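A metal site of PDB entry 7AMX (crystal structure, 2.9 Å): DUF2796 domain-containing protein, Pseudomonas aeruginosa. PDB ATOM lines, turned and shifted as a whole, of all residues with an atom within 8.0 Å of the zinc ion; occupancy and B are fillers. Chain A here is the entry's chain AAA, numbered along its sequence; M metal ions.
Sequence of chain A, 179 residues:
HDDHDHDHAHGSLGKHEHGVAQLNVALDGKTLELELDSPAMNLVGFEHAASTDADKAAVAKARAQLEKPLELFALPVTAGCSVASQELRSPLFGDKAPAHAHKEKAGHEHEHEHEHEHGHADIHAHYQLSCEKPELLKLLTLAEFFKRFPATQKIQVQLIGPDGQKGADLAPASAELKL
N of Ala 121 sits close to OE1 of Glu 47, 3.0 Å away. The side-chain carboxylate (OE2) of Glu 47 sits at hydrogen-bond distance from the backbone NH (N) of Ala 40, 3.4 Å away. A ring nitrogen (ND1) of His 16 sits at hydrogen-bond distance from the side-chain carboxylate of Asp 122 (2.7 Å). The side-chain carboxylate (OE2) of Glu 47 lies within hydrogen-bond range of the backbone NH (N) of Met 41.
The zinc ion is bound by a ring nitrogen (NE2) of His 16 (1.9 Å), the side-chain carboxylate of Glu 47 (2.0 Å), a ring nitrogen (ND1) of His 120 (2.1 Å) and a ring nitrogen (NE2) of His 18 (2.1 Å). The zinc ion has four donor atoms within binding distance.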
ATOM      1  N   HIS A  16      -8.117   3.883  -9.653  1.00  0.00           N
ATOM      2  CA  HIS A  16      -8.291   3.090  -8.405  1.00  0.00           C
ATOM      3  C   HIS A  16      -8.619   4.076  -7.286  1.00  0.00           C
ATOM      4  O   HIS A  16      -7.708   4.487  -6.569  1.00  0.00           O
ATOM      5  CB  HIS A  16      -7.060   2.222  -8.161  1.00  0.00           C
ATOM      6  CG  HIS A  16      -7.130   1.385  -6.929  1.00  0.00           C
ATOM      7  ND1 HIS A  16      -7.144   0.002  -7.005  1.00  0.00           N
ATOM      8  CD2 HIS A  16      -7.134   1.693  -5.612  1.00  0.00           C
ATOM      9  CE1 HIS A  16      -7.163  -0.501  -5.783  1.00  0.00           C
ATOM     10  NE2 HIS A  16      -7.175   0.515  -4.903  1.00  0.00           N
ATOM     11  N   GLU A  17      -9.881   4.495  -7.222  1.00  0.00           N
ATOM     12  CA  GLU A  17     -10.479   5.338  -6.149  1.00  0.00           C
ATOM     13  C   GLU A  17     -11.354   4.447  -5.246  1.00  0.00           C
ATOM     14  O   GLU A  17     -12.403   3.991  -5.716  1.00  0.00           O
ATOM     15  CB  GLU A  17     -11.257   6.477  -6.806  1.00  0.00           C
ATOM     16  CG  GLU A  17     -11.477   7.663  -5.891  1.00  0.00           C
ATOM     17  CD  GLU A  17     -12.208   8.835  -6.539  1.00  0.00           C
ATOM     18  OE1 GLU A  17     -12.608   8.720  -7.724  1.00  0.00           O
ATOM     19  OE2 GLU A  17     -12.383   9.875  -5.861  1.00  0.00           O
ATOM     20  N   HIS A  18     -10.926   4.191  -4.003  1.00  0.00           N
ATOM     21  CA  HIS A  18     -11.690   3.406  -2.997  1.00  0.00           C
ATOM     22  C   HIS A  18     -13.096   4.000  -2.905  1.00  0.00           C
ATOM     23  O   HIS A  18     -13.185   5.225  -2.810  1.00  0.00           O
ATOM     24  CB  HIS A  18     -10.975   3.405  -1.651  1.00  0.00           C
ATOM     25  CG  HIS A  18      -9.661   2.709  -1.694  1.00  0.00           C
ATOM     26  ND1 HIS A  18      -9.056   2.247  -0.562  1.00  0.00           N
ATOM     27  CD2 HIS A  18      -8.853   2.359  -2.728  1.00  0.00           C
ATOM     28  CE1 HIS A  18      -7.922   1.656  -0.873  1.00  0.00           C
ATOM     29  NE2 HIS A  18      -7.776   1.703  -2.197  1.00  0.00           N
ATOM     30  N   SER A  38     -13.201  -2.862 -10.072  1.00  0.00           N
ATOM     31  CA  SER A  38     -13.407  -2.317  -8.716  1.00  0.00           C
ATOM     32  C   SER A  38     -12.166  -2.557  -7.869  1.00  0.00           C
ATOM     33  O   SER A  38     -11.606  -3.650  -7.901  1.00  0.00           O
ATOM     34  CB  SER A  38     -14.607  -2.963  -8.088  1.00  0.00           C
ATOM     35  OG  SER A  38     -14.987  -2.290  -6.909  1.00  0.00           O
ATOM     36  N   PRO A  39     -11.680  -1.561  -7.100  1.00  0.00           N
ATOM     37  CA  PRO A  39     -10.833  -1.865  -5.950  1.00  0.00           C
ATOM     38  C   PRO A  39     -11.583  -2.864  -5.042  1.00  0.00           C
ATOM     39  O   PRO A  39     -12.764  -2.770  -4.911  1.00  0.00           O
ATOM     40  CB  PRO A  39     -10.563  -0.506  -5.280  1.00  0.00           C
ATOM     41  CG  PRO A  39     -11.551   0.444  -5.925  1.00  0.00           C
ATOM     42  CD  PRO A  39     -11.909  -0.130  -7.289  1.00  0.00           C
ATOM     43  N   ALA A  40     -10.880  -3.811  -4.447  1.00  0.00           N
ATOM     44  CA  ALA A  40     -11.455  -4.801  -3.525  1.00  0.00           C
ATOM     45  C   ALA A  40     -11.980  -4.137  -2.234  1.00  0.00           C
ATOM     46  O   ALA A  40     -12.925  -4.692  -1.607  1.00  0.00           O
ATOM     47  CB  ALA A  40     -10.377  -5.801  -3.230  1.00  0.00           C
ATOM     48  N   MET A  41     -11.410  -3.002  -1.818  1.00  0.00           N
ATOM     49  CA  MET A  41     -11.833  -2.277  -0.591  1.00  0.00           C
ATOM     50  C   MET A  41     -13.367  -2.192  -0.496  1.00  0.00           C
ATOM     51  O   MET A  41     -13.866  -2.273   0.619  1.00  0.00           O
ATOM     52  CB  MET A  41     -11.239  -0.862  -0.539  1.00  0.00           C
ATOM     53  CG  MET A  41     -10.995  -0.368   0.895  1.00  0.00           C
ATOM     54  SD  MET A  41      -9.487  -1.063   1.649  1.00  0.00           S
ATOM     55  CE  MET A  41     -10.030  -1.331   3.333  1.00  0.00           C
ATOM     56  N   ASN A  42     -14.112  -2.035  -1.602  1.00  0.00           N
ATOM     57  CA  ASN A  42     -15.593  -1.836  -1.565  1.00  0.00           C
ATOM     58  C   ASN A  42     -16.322  -3.168  -1.653  1.00  0.00           C
ATOM     59  O   ASN A  42     -17.592  -3.143  -1.635  1.00  0.00           O
ATOM     60  CB  ASN A  42     -16.179  -1.063  -2.739  1.00  0.00           C
ATOM     61  CG  ASN A  42     -15.138  -0.329  -3.535  1.00  0.00           C
ATOM     62  OD1 ASN A  42     -14.196   0.203  -2.953  1.00  0.00           O
ATOM     63  ND2 ASN A  42     -15.290  -0.301  -4.842  1.00  0.00           N
ATOM     64  N   PHE A  46     -10.945  -4.844   2.374  1.00  0.00           N
ATOM     65  CA  PHE A  46      -9.475  -4.779   2.485  1.00  0.00           C
ATOM     66  C   PHE A  46      -8.854  -5.046   1.120  1.00  0.00           C
ATOM     67  O   PHE A  46      -9.588  -5.172   0.127  1.00  0.00           O
ATOM     68  CB  PHE A  46      -8.954  -5.746   3.544  1.00  0.00           C
ATOM     69  CG  PHE A  46      -9.319  -7.195   3.362  1.00  0.00           C
ATOM     70  CD1 PHE A  46      -8.524  -8.030   2.585  1.00  0.00           C
ATOM     71  CD2 PHE A  46     -10.396  -7.735   4.036  1.00  0.00           C
ATOM     72  CE1 PHE A  46      -8.829  -9.377   2.455  1.00  0.00           C
ATOM     73  CE2 PHE A  46     -10.719  -9.082   3.892  1.00  0.00           C
ATOM     74  CZ  PHE A  46      -9.935  -9.903   3.102  1.00  0.00           C
ATOM     75  N   GLU A  47      -7.524  -5.024   1.067  1.00  0.00           N
ATOM     76  CA  GLU A  47      -6.732  -5.253  -0.159  1.00  0.00           C
ATOM     77  C   GLU A  47      -5.439  -6.017   0.191  1.00  0.00           C
ATOM     78  O   GLU A  47      -4.787  -6.509  -0.739  1.00  0.00           O
ATOM     79  CB  GLU A  47      -6.463  -3.926  -0.855  1.00  0.00           C
ATOM     80  CG  GLU A  47      -7.739  -3.176  -1.205  1.00  0.00           C
ATOM     81  CD  GLU A  47      -7.610  -2.151  -2.316  1.00  0.00           C
ATOM     82  OE1 GLU A  47      -6.466  -1.700  -2.607  1.00  0.00           O
ATOM     83  OE2 GLU A  47      -8.672  -1.807  -2.890  1.00  0.00           O
ATOM     84  N   GLY A 119       0.638  -2.421  -1.920  1.00  0.00           N
ATOM     85  CA  GLY A 119      -0.304  -3.534  -1.768  1.00  0.00           C
ATOM     86  C   GLY A 119      -1.772  -3.092  -1.861  1.00  0.00           C
ATOM     87  O   GLY A 119      -2.520  -3.266  -0.871  1.00  0.00           O
ATOM     88  N   HIS A 120      -2.151  -2.517  -3.014  1.00  0.00           N
ATOM     89  CA  HIS A 120      -3.560  -2.281  -3.469  1.00  0.00           C
ATOM     90  C   HIS A 120      -3.989  -3.463  -4.352  1.00  0.00           C
ATOM     91  O   HIS A 120      -3.115  -4.093  -4.927  1.00  0.00           O
ATOM     92  CB  HIS A 120      -3.666  -0.951  -4.225  1.00  0.00           C
ATOM     93  CG  HIS A 120      -3.624   0.267  -3.365  1.00  0.00           C
ATOM     94  ND1 HIS A 120      -4.668   0.626  -2.543  1.00  0.00           N
ATOM     95  CD2 HIS A 120      -2.693   1.240  -3.251  1.00  0.00           C
ATOM     96  CE1 HIS A 120      -4.362   1.742  -1.915  1.00  0.00           C
ATOM     97  NE2 HIS A 120      -3.165   2.150  -2.349  1.00  0.00           N
ATOM     98  N   ALA A 121      -5.283  -3.749  -4.475  1.00  0.00           N
ATOM     99  CA  ALA A 121      -5.825  -4.942  -5.188  1.00  0.00           C
ATOM    100  C   ALA A 121      -7.171  -4.618  -5.832  1.00  0.00           C
ATOM    101  O   ALA A 121      -8.007  -3.957  -5.177  1.00  0.00           O
ATOM    102  CB  ALA A 121      -5.926  -6.120  -4.251  1.00  0.00           C
ATOM    103  N   ASP A 122      -7.348  -5.047  -7.079  1.00  0.00           N
ATOM    104  CA  ASP A 122      -8.570  -4.793  -7.897  1.00  0.00           C
ATOM    105  C   ASP A 122      -9.375  -6.088  -7.935  1.00  0.00           C
ATOM    106  O   ASP A 122      -8.833  -7.124  -7.500  1.00  0.00           O
ATOM    107  CB  ASP A 122      -8.207  -4.307  -9.312  1.00  0.00           C
ATOM    108  CG  ASP A 122      -8.088  -2.795  -9.481  1.00  0.00           C
ATOM    109  OD1 ASP A 122      -7.513  -2.154  -8.586  1.00  0.00           O
ATOM    110  OD2 ASP A 122      -8.577  -2.282 -10.527  1.00  0.00           O
HETATM  111 ZN    ZN M   1      -6.596   0.263  -3.146  1.00  0.00          ZN
